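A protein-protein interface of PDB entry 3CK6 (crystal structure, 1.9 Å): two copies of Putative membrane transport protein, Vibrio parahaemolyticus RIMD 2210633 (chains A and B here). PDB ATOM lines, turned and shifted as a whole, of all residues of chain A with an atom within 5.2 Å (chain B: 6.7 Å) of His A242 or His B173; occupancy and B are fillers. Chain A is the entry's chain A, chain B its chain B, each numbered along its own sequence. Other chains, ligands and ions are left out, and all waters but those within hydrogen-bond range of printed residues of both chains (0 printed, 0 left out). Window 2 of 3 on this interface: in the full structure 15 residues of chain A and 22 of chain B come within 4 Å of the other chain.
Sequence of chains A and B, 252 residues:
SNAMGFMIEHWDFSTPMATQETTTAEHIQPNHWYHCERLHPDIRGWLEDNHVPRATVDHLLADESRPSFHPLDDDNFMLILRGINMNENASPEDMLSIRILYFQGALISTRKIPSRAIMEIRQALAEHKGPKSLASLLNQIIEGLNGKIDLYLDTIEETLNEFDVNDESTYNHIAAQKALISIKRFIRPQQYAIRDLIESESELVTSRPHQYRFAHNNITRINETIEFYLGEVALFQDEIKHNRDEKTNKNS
The side-chain amino group of Lys B178 lies within salt-bridge range of the side-chain carboxylate of Glu A239 (2.8 Å). The side-chain carboxylate (OE2) of Glu A246 lies within salt-bridge range of the guanidinium group (NE) of Arg B244 (3.6 Å). A ring nitrogen (ND1) of His A242 sits at hydrogen-bond distance from the guanidinium group (NH2) of Arg B244 (2.9 Å).
O of Lys A241 sits close to OD2 of Asp A245, at 2.6 Å.
CA of Glu A239 touches CD1 of Ile B174 (3.6 Å). CE1 of His A242 touches CD2 of Tyr B171, 3.3 Å away. His B173 touches His A242. His A242 touches Ile B174 (CB to CD1, 3.96 Å). CB of Asp A245 touches NE of Arg B244, 3.5 Å away. CG of Glu B168 touches OE1 of Glu A246, 3.5 Å away. Glu A246 touches Tyr B171 (OE2 to CE2, 3.7 Å).
Ile A240 touches none of the printed residues of chain B. His A242 touches just these residues of chain B: Tyr B171 (3.3 Å), His B173 (3.4 Å), Ile B174 (3.96 Å) and Arg B244 (2.9 Å). Of the printed residues of chain A, Glu B168 touches Glu A246 (3.5 Å). Printed residues of chain A within 4 Å of Tyr B171: His A242 and Glu A246. His B173 touches one residue of chain A. Of the printed residues of chain A, Arg B244 touches His A242 (2.9 Å), Asp A245 (3.5 Å) and Glu A246 (3.6 Å). The nearest residue of chain B that does not touch His A242 is Ile B240 (4.3 Å). The nearest printed residue of chain A that does not touch His B173 is Asp A238 (6.6 Å).
Of the 10 printed residues of chain A, 4 touch a printed residue of chain B. Hydrophobic or aromatic side chains of chain A that line the printed part of chain B: His A242. Among the printed residues, 10 pairs touch across the chains.
Positions printed for both chains: 240 and 244. Of the 10 pairs that touch across the chains among the printed residues, none has its exchanged pair printed and touching as well.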
ATOM      1  N   ASP A 238     -32.477   2.023  -8.655  1.00  0.00           N
ATOM      2  CA  ASP A 238     -32.357   0.601  -8.947  1.00  0.00           C
ATOM      3  C   ASP A 238     -31.889  -0.141  -7.698  1.00  0.00           C
ATOM      4  O   ASP A 238     -32.395  -1.222  -7.387  1.00  0.00           O
ATOM      5  CB  ASP A 238     -31.378   0.346 -10.103  1.00  0.00           C
ATOM      6  CG  ASP A 238     -31.955   0.720 -11.475  1.00  0.00           C
ATOM      7  OD1 ASP A 238     -31.160   0.784 -12.441  1.00  0.00           O
ATOM      8  OD2 ASP A 238     -33.187   0.936 -11.603  1.00  0.00           O
ATOM      9  N   GLU A 239     -30.925   0.456  -6.991  1.00  0.00           N
ATOM     10  CA  GLU A 239     -30.419  -0.097  -5.737  1.00  0.00           C
ATOM     11  C   GLU A 239     -31.563  -0.353  -4.756  1.00  0.00           C
ATOM     12  O   GLU A 239     -31.688  -1.460  -4.237  1.00  0.00           O
ATOM     13  CB  GLU A 239     -29.365   0.825  -5.116  1.00  0.00           C
ATOM     14  CG  GLU A 239     -28.447   0.139  -4.104  1.00  0.00           C
ATOM     15  CD  GLU A 239     -27.291   1.032  -3.637  1.00  0.00           C
ATOM     16  OE1 GLU A 239     -26.944   2.003  -4.344  1.00  0.00           O
ATOM     17  OE2 GLU A 239     -26.722   0.750  -2.554  1.00  0.00           O
ATOM     18  N   ILE A 240     -32.398   0.662  -4.523  1.00  0.00           N
ATOM     19  CA  ILE A 240     -33.577   0.514  -3.655  1.00  0.00           C
ATOM     20  C   ILE A 240     -34.486  -0.635  -4.127  1.00  0.00           C
ATOM     21  O   ILE A 240     -34.943  -1.458  -3.306  1.00  0.00           O
ATOM     22  CB  ILE A 240     -34.403   1.823  -3.561  1.00  0.00           C
ATOM     23  CG1 ILE A 240     -33.549   2.980  -3.049  1.00  0.00           C
ATOM     24  CG2 ILE A 240     -35.605   1.648  -2.635  1.00  0.00           C
ATOM     25  CD1 ILE A 240     -34.159   4.339  -3.347  1.00  0.00           C
ATOM     26  N   LYS A 241     -34.745  -0.696  -5.438  1.00  0.00           N
ATOM     27  CA  LYS A 241     -35.606  -1.754  -6.014  1.00  0.00           C
ATOM     28  C   LYS A 241     -35.026  -3.162  -5.869  1.00  0.00           C
ATOM     29  O   LYS A 241     -35.766  -4.125  -5.676  1.00  0.00           O
ATOM     30  CB  LYS A 241     -35.953  -1.471  -7.481  1.00  0.00           C
ATOM     31  CG  LYS A 241     -37.061  -0.438  -7.663  1.00  0.00           C
ATOM     32  CD  LYS A 241     -36.889   0.386  -8.935  1.00  0.00           C
ATOM     33  CE  LYS A 241     -37.620   1.727  -8.822  1.00  0.00           C
ATOM     34  NZ  LYS A 241     -37.103   2.588  -7.693  1.00  0.00           N
ATOM     35  N   HIS A 242     -33.705  -3.280  -5.981  1.00  0.00           N
ATOM     36  CA  HIS A 242     -33.035  -4.560  -5.771  1.00  0.00           C
ATOM     37  C   HIS A 242     -33.055  -4.950  -4.292  1.00  0.00           C
ATOM     38  O   HIS A 242     -33.350  -6.098  -3.953  1.00  0.00           O
ATOM     39  CB  HIS A 242     -31.599  -4.530  -6.307  1.00  0.00           C
ATOM     40  CG  HIS A 242     -30.860  -5.821  -6.119  1.00  0.00           C
ATOM     41  ND1 HIS A 242     -31.132  -6.949  -6.863  1.00  0.00           N
ATOM     42  CD2 HIS A 242     -29.865  -6.164  -5.266  1.00  0.00           C
ATOM     43  CE1 HIS A 242     -30.338  -7.932  -6.478  1.00  0.00           C
ATOM     44  NE2 HIS A 242     -29.559  -7.483  -5.509  1.00  0.00           N
ATOM     45  N   ASN A 243     -32.748  -3.988  -3.421  1.00  0.00           N
ATOM     46  CA  ASN A 243     -32.715  -4.224  -1.976  1.00  0.00           C
ATOM     47  C   ASN A 243     -34.071  -4.657  -1.403  1.00  0.00           C
ATOM     48  O   ASN A 243     -34.153  -5.613  -0.613  1.00  0.00           O
ATOM     49  CB  ASN A 243     -32.204  -2.974  -1.253  1.00  0.00           C
ATOM     50  CG  ASN A 243     -32.107  -3.162   0.250  1.00  0.00           C
ATOM     51  OD1 ASN A 243     -31.242  -3.886   0.746  1.00  0.00           O
ATOM     52  ND2 ASN A 243     -32.989  -2.495   0.986  1.00  0.00           N
ATOM     53  N   ARG A 244     -35.130  -3.961  -1.819  1.00  0.00           N
ATOM     54  CA  ARG A 244     -36.490  -4.251  -1.354  1.00  0.00           C
ATOM     55  C   ARG A 244     -36.989  -5.630  -1.800  1.00  0.00           C
ATOM     56  O   ARG A 244     -37.655  -6.339  -1.032  1.00  0.00           O
ATOM     57  CB  ARG A 244     -37.460  -3.163  -1.814  1.00  0.00           C
ATOM     58  CG  ARG A 244     -38.501  -2.835  -0.776  1.00  0.00           C
ATOM     59  CD  ARG A 244     -39.886  -2.743  -1.376  1.00  0.00           C
ATOM     60  NE  ARG A 244     -40.901  -2.584  -0.331  1.00  0.00           N
ATOM     61  CZ  ARG A 244     -41.534  -3.580   0.289  1.00  0.00           C
ATOM     62  NH1 ARG A 244     -41.283  -4.851  -0.014  1.00  0.00           N
ATOM     63  NH2 ARG A 244     -42.434  -3.297   1.219  1.00  0.00           N
ATOM     64  N   ASP A 245     -36.656  -6.006  -3.032  1.00  0.00           N
ATOM     65  CA  ASP A 245     -37.019  -7.314  -3.577  1.00  0.00           C
ATOM     66  C   ASP A 245     -36.155  -8.465  -3.039  1.00  0.00           C
ATOM     67  O   ASP A 245     -36.569  -9.633  -3.081  1.00  0.00           O
ATOM     68  CB  ASP A 245     -36.978  -7.281  -5.103  1.00  0.00           C
ATOM     69  CG  ASP A 245     -38.159  -6.538  -5.703  1.00  0.00           C
ATOM     70  OD1 ASP A 245     -39.128  -7.208  -6.117  1.00  0.00           O
ATOM     71  OD2 ASP A 245     -38.126  -5.288  -5.756  1.00  0.00           O
ATOM     72  N   GLU A 246     -34.964  -8.132  -2.536  1.00  0.00           N
ATOM     73  CA  GLU A 246     -34.051  -9.118  -1.934  1.00  0.00           C
ATOM     74  C   GLU A 246     -34.229  -9.284  -0.415  1.00  0.00           C
ATOM     75  O   GLU A 246     -33.861 -10.326   0.137  1.00  0.00           O
ATOM     76  CB  GLU A 246     -32.581  -8.803  -2.260  1.00  0.00           C
ATOM     77  CG  GLU A 246     -32.188  -8.947  -3.739  1.00  0.00           C
ATOM     78  CD  GLU A 246     -32.108 -10.392  -4.223  1.00  0.00           C
ATOM     79  OE1 GLU A 246     -31.424 -11.221  -3.572  1.00  0.00           O
ATOM     80  OE2 GLU A 246     -32.720 -10.694  -5.275  1.00  0.00           O
ATOM     81  N   LYS A 247     -34.781  -8.267   0.257  1.00  0.00           N
ATOM     82  CA  LYS A 247     -35.002  -8.348   1.711  1.00  0.00           C
ATOM     83  C   LYS A 247     -36.445  -8.721   2.093  1.00  0.00           C
ATOM     84  O   LYS A 247     -37.318  -8.892   1.226  1.00  0.00           O
ATOM     85  CB  LYS A 247     -34.554  -7.058   2.422  1.00  0.00           C
ATOM     86  CG  LYS A 247     -35.655  -6.035   2.674  1.00  0.00           C
ATOM     87  CD  LYS A 247     -35.074  -4.706   3.136  1.00  0.00           C
ATOM     88  CE  LYS A 247     -36.108  -3.587   3.044  1.00  0.00           C
ATOM     89  NZ  LYS A 247     -35.459  -2.239   3.010  1.00  0.00           N
ATOM     90  N   THR B 159     -15.809  -9.436 -12.664  1.00  0.00           N
ATOM     91  CA  THR B 159     -17.014  -9.302 -11.836  1.00  0.00           C
ATOM     92  C   THR B 159     -18.265  -9.675 -12.627  1.00  0.00           C
ATOM     93  O   THR B 159     -19.092 -10.466 -12.168  1.00  0.00           O
ATOM     94  CB  THR B 159     -17.150  -7.872 -11.247  1.00  0.00           C
ATOM     95  OG1 THR B 159     -16.032  -7.609 -10.399  1.00  0.00           O
ATOM     96  CG2 THR B 159     -18.440  -7.726 -10.432  1.00  0.00           C
ATOM     97  N   LEU B 160     -18.393  -9.104 -13.818  1.00  0.00           N
ATOM     98  CA  LEU B 160     -19.477  -9.444 -14.742  1.00  0.00           C
ATOM     99  C   LEU B 160     -19.469 -10.921 -15.150  1.00  0.00           C
ATOM    100  O   LEU B 160     -20.536 -11.532 -15.272  1.00  0.00           O
ATOM    101  CB  LEU B 160     -19.423  -8.560 -15.994  1.00  0.00           C
ATOM    102  CG  LEU B 160     -19.987  -7.128 -16.031  1.00  0.00           C
ATOM    103  CD1 LEU B 160     -19.807  -6.351 -14.727  1.00  0.00           C
ATOM    104  CD2 LEU B 160     -19.349  -6.401 -17.182  1.00  0.00           C
ATOM    105  N   PHE B 163     -21.304 -13.183 -12.664  1.00  0.00           N
ATOM    106  CA  PHE B 163     -22.758 -13.021 -12.555  1.00  0.00           C
ATOM    107  C   PHE B 163     -23.432 -14.382 -12.738  1.00  0.00           C
ATOM    108  O   PHE B 163     -23.309 -14.986 -13.807  1.00  0.00           O
ATOM    109  CB  PHE B 163     -23.302 -12.070 -13.638  1.00  0.00           C
ATOM    110  CG  PHE B 163     -23.100 -10.596 -13.357  1.00  0.00           C
ATOM    111  CD1 PHE B 163     -22.837 -10.126 -12.069  1.00  0.00           C
ATOM    112  CD2 PHE B 163     -23.204  -9.664 -14.407  1.00  0.00           C
ATOM    113  CE1 PHE B 163     -22.665  -8.762 -11.822  1.00  0.00           C
ATOM    114  CE2 PHE B 163     -23.038  -8.300 -14.168  1.00  0.00           C
ATOM    115  CZ  PHE B 163     -22.763  -7.846 -12.874  1.00  0.00           C
ATOM    116  N   GLU B 168     -27.012 -15.607  -5.343  1.00  0.00           N
ATOM    117  CA  GLU B 168     -27.156 -14.269  -4.746  1.00  0.00           C
ATOM    118  C   GLU B 168     -25.849 -13.571  -4.418  1.00  0.00           C
ATOM    119  O   GLU B 168     -25.759 -12.339  -4.482  1.00  0.00           O
ATOM    120  CB  GLU B 168     -27.949 -14.364  -3.446  1.00  0.00           C
ATOM    121  CG  GLU B 168     -29.408 -14.040  -3.559  1.00  0.00           C
ATOM    122  CD  GLU B 168     -30.124 -14.322  -2.258  1.00  0.00           C
ATOM    123  OE1 GLU B 168     -30.941 -15.271  -2.229  1.00  0.00           O
ATOM    124  OE2 GLU B 168     -29.836 -13.618  -1.261  1.00  0.00           O
ATOM    125  N   THR B 170     -23.249 -13.396  -5.988  1.00  0.00           N
ATOM    126  CA  THR B 170     -22.596 -12.880  -7.201  1.00  0.00           C
ATOM    127  C   THR B 170     -23.232 -11.580  -7.706  1.00  0.00           C
ATOM    128  O   THR B 170     -22.860 -11.066  -8.770  1.00  0.00           O
ATOM    129  CB  THR B 170     -22.609 -13.917  -8.364  1.00  0.00           C
ATOM    130  OG1 THR B 170     -23.939 -14.058  -8.883  1.00  0.00           O
ATOM    131  CG2 THR B 170     -22.082 -15.282  -7.909  1.00  0.00           C
ATOM    132  N   TYR B 171     -24.178 -11.056  -6.928  1.00  0.00           N
ATOM    133  CA  TYR B 171     -25.014  -9.922  -7.326  1.00  0.00           C
ATOM    134  C   TYR B 171     -24.300  -8.610  -7.021  1.00  0.00           C
ATOM    135  O   TYR B 171     -24.767  -7.808  -6.205  1.00  0.00           O
ATOM    136  CB  TYR B 171     -26.368  -9.963  -6.600  1.00  0.00           C
ATOM    137  CG  TYR B 171     -27.389 -10.989  -7.079  1.00  0.00           C
ATOM    138  CD1 TYR B 171     -27.016 -12.139  -7.784  1.00  0.00           C
ATOM    139  CD2 TYR B 171     -28.738 -10.823  -6.777  1.00  0.00           C
ATOM    140  CE1 TYR B 171     -27.977 -13.088  -8.192  1.00  0.00           C
ATOM    141  CE2 TYR B 171     -29.697 -11.757  -7.171  1.00  0.00           C
ATOM    142  CZ  TYR B 171     -29.314 -12.881  -7.878  1.00  0.00           C
ATOM    143  OH  TYR B 171     -30.283 -13.774  -8.268  1.00  0.00           O
ATOM    144  N   ASN B 172     -23.164  -8.408  -7.678  1.00  0.00           N
ATOM    145  CA  ASN B 172     -22.347  -7.206  -7.498  1.00  0.00           C
ATOM    146  C   ASN B 172     -22.548  -6.228  -8.647  1.00  0.00           C
ATOM    147  O   ASN B 172     -21.659  -5.436  -8.966  1.00  0.00           O
ATOM    148  CB  ASN B 172     -20.871  -7.596  -7.357  1.00  0.00           C
ATOM    149  CG  ASN B 172     -20.641  -8.596  -6.226  1.00  0.00           C
ATOM    150  OD1 ASN B 172     -20.818  -8.269  -5.051  1.00  0.00           O
ATOM    151  ND2 ASN B 172     -20.266  -9.825  -6.580  1.00  0.00           N
ATOM    152  N   HIS B 173     -23.737  -6.284  -9.244  1.00  0.00           N
ATOM    153  CA  HIS B 173     -24.057  -5.538 -10.463  1.00  0.00           C
ATOM    154  C   HIS B 173     -24.193  -4.039 -10.227  1.00  0.00           C
ATOM    155  O   HIS B 173     -23.918  -3.247 -11.114  1.00  0.00           O
ATOM    156  CB  HIS B 173     -25.324  -6.092 -11.140  1.00  0.00           C
ATOM    157  CG  HIS B 173     -26.431  -6.421 -10.185  1.00  0.00           C
ATOM    158  ND1 HIS B 173     -27.473  -5.556  -9.921  1.00  0.00           N
ATOM    159  CD2 HIS B 173     -26.652  -7.514  -9.421  1.00  0.00           C
ATOM    160  CE1 HIS B 173     -28.290  -6.105  -9.041  1.00  0.00           C
ATOM    161  NE2 HIS B 173     -27.817  -7.296  -8.720  1.00  0.00           N
ATOM    162  N   ILE B 174     -24.635  -3.660  -9.032  1.00  0.00           N
ATOM    163  CA  ILE B 174     -24.801  -2.249  -8.714  1.00  0.00           C
ATOM    164  C   ILE B 174     -23.447  -1.572  -8.520  1.00  0.00           C
ATOM    165  O   ILE B 174     -23.236  -0.484  -9.050  1.00  0.00           O
ATOM    166  CB  ILE B 174     -25.782  -2.026  -7.537  1.00  0.00           C
ATOM    167  CG1 ILE B 174     -27.227  -2.169  -8.041  1.00  0.00           C
ATOM    168  CG2 ILE B 174     -25.600  -0.644  -6.913  1.00  0.00           C
ATOM    169  CD1 ILE B 174     -28.200  -2.612  -6.979  1.00  0.00           C
ATOM    170  N   ALA B 175     -22.532  -2.243  -7.817  1.00  0.00           N
ATOM    171  CA  ALA B 175     -21.135  -1.793  -7.686  1.00  0.00           C
ATOM    172  C   ALA B 175     -20.443  -1.611  -9.034  1.00  0.00           C
ATOM    173  O   ALA B 175     -19.752  -0.610  -9.254  1.00  0.00           O
ATOM    174  CB  ALA B 175     -20.338  -2.766  -6.818  1.00  0.00           C
ATOM    175  N   ALA B 176     -20.636  -2.586  -9.928  1.00  0.00           N
ATOM    176  CA  ALA B 176     -20.071  -2.555 -11.282  1.00  0.00           C
ATOM    177  C   ALA B 176     -20.556  -1.324 -12.055  1.00  0.00           C
ATOM    178  O   ALA B 176     -19.752  -0.581 -12.588  1.00  0.00           O
ATOM    179  CB  ALA B 176     -20.425  -3.838 -12.034  1.00  0.00           C
ATOM    180  N   GLN B 177     -21.877  -1.126 -12.089  1.00  0.00           N
ATOM    181  CA  GLN B 177     -22.506   0.022 -12.735  1.00  0.00           C
ATOM    182  C   GLN B 177     -22.003   1.367 -12.218  1.00  0.00           C
ATOM    183  O   GLN B 177     -21.712   2.262 -13.030  1.00  0.00           O
ATOM    184  CB  GLN B 177     -24.022  -0.034 -12.586  1.00  0.00           C
ATOM    185  CG  GLN B 177     -24.755   0.970 -13.481  1.00  0.00           C
ATOM    186  CD  GLN B 177     -26.273   0.790 -13.458  1.00  0.00           C
ATOM    187  OE1 GLN B 177     -27.013   1.629 -13.992  1.00  0.00           O
ATOM    188  NE2 GLN B 177     -26.742  -0.301 -12.848  1.00  0.00           N
ATOM    189  N   LYS B 178     -21.921   1.501 -10.890  1.00  0.00           N
ATOM    190  CA  LYS B 178     -21.355   2.704 -10.234  1.00  0.00           C
ATOM    191  C   LYS B 178     -19.973   3.047 -10.783  1.00  0.00           C
ATOM    192  O   LYS B 178     -19.689   4.202 -11.106  1.00  0.00           O
ATOM    193  CB  LYS B 178     -21.254   2.529  -8.698  1.00  0.00           C
ATOM    194  CG  LYS B 178     -22.581   2.453  -7.933  1.00  0.00           C
ATOM    195  CD  LYS B 178     -22.464   2.983  -6.477  1.00  0.00           C
ATOM    196  CE  LYS B 178     -23.825   3.051  -5.748  1.00  0.00           C
ATOM    197  NZ  LYS B 178     -24.201   1.821  -4.964  1.00  0.00           N
ATOM    198  N   VAL B 233     -24.491  -5.324 -17.585  1.00  0.00           N
ATOM    199  CA  VAL B 233     -25.084  -5.032 -16.265  1.00  0.00           C
ATOM    200  C   VAL B 233     -26.604  -4.906 -16.336  1.00  0.00           C
ATOM    201  O   VAL B 233     -27.312  -5.450 -15.487  1.00  0.00           O
ATOM    202  CB  VAL B 233     -24.487  -3.764 -15.615  1.00  0.00           C
ATOM    203  CG1 VAL B 233     -25.318  -3.333 -14.398  1.00  0.00           C
ATOM    204  CG2 VAL B 233     -23.028  -4.017 -15.214  1.00  0.00           C
ATOM    205  N   PHE B 236     -28.189  -8.434 -16.774  1.00  0.00           N
ATOM    206  CA  PHE B 236     -28.209  -9.217 -15.531  1.00  0.00           C
ATOM    207  C   PHE B 236     -29.331  -8.770 -14.593  1.00  0.00           C
ATOM    208  O   PHE B 236     -30.013  -9.606 -13.961  1.00  0.00           O
ATOM    209  CB  PHE B 236     -26.849  -9.186 -14.808  1.00  0.00           C
ATOM    210  CG  PHE B 236     -26.752 -10.189 -13.671  1.00  0.00           C
ATOM    211  CD1 PHE B 236     -27.180 -11.512 -13.848  1.00  0.00           C
ATOM    212  CD2 PHE B 236     -26.240  -9.817 -12.428  1.00  0.00           C
ATOM    213  CE1 PHE B 236     -27.116 -12.444 -12.805  1.00  0.00           C
ATOM    214  CE2 PHE B 236     -26.166 -10.754 -11.374  1.00  0.00           C
ATOM    215  CZ  PHE B 236     -26.608 -12.065 -11.569  1.00  0.00           C
ATOM    216  N   GLN B 237     -29.540  -7.457 -14.534  1.00  0.00           N
ATOM    217  CA  GLN B 237     -30.625  -6.861 -13.756  1.00  0.00           C
ATOM    218  C   GLN B 237     -32.003  -7.330 -14.219  1.00  0.00           C
ATOM    219  O   GLN B 237     -32.874  -7.590 -13.386  1.00  0.00           O
ATOM    220  CB  GLN B 237     -30.508  -5.330 -13.736  1.00  0.00           C
ATOM    221  CG  GLN B 237     -29.345  -4.841 -12.881  1.00  0.00           C
ATOM    222  CD  GLN B 237     -29.153  -3.325 -12.889  1.00  0.00           C
ATOM    223  OE1 GLN B 237     -28.718  -2.744 -11.888  1.00  0.00           O
ATOM    224  NE2 GLN B 237     -29.460  -2.681 -14.017  1.00  0.00           N
ATOM    225  N   ILE B 240     -32.270 -11.146 -13.224  1.00  0.00           N
ATOM    226  CA  ILE B 240     -32.655 -11.232 -11.811  1.00  0.00           C
ATOM    227  C   ILE B 240     -34.153 -10.973 -11.617  1.00  0.00           C
ATOM    228  O   ILE B 240     -34.859 -11.787 -11.001  1.00  0.00           O
ATOM    229  CB  ILE B 240     -31.834 -10.252 -10.937  1.00  0.00           C
ATOM    230  CG1 ILE B 240     -30.350 -10.615 -10.980  1.00  0.00           C
ATOM    231  CG2 ILE B 240     -32.330 -10.267  -9.487  1.00  0.00           C
ATOM    232  CD1 ILE B 240     -29.444  -9.518 -10.474  1.00  0.00           C
ATOM    233  N   ARG B 244     -37.026 -13.505 -10.256  1.00  0.00           N
ATOM    234  CA  ARG B 244     -37.838 -13.185  -9.072  1.00  0.00           C
ATOM    235  C   ARG B 244     -39.324 -13.514  -9.233  1.00  0.00           C
ATOM    236  O   ARG B 244     -39.967 -13.951  -8.280  1.00  0.00           O
ATOM    237  CB  ARG B 244     -37.706 -11.707  -8.693  1.00  0.00           C
ATOM    238  CG  ARG B 244     -36.392 -11.315  -8.042  1.00  0.00           C
ATOM    239  CD  ARG B 244     -36.503  -9.935  -7.413  1.00  0.00           C
ATOM    240  NE  ARG B 244     -35.215  -9.244  -7.351  1.00  0.00           N
ATOM    241  CZ  ARG B 244     -34.901  -8.148  -8.050  1.00  0.00           C
ATOM    242  NH1 ARG B 244     -35.779  -7.584  -8.874  1.00  0.00           N
ATOM    243  NH2 ARG B 244     -33.700  -7.607  -7.922  1.00  0.00           N
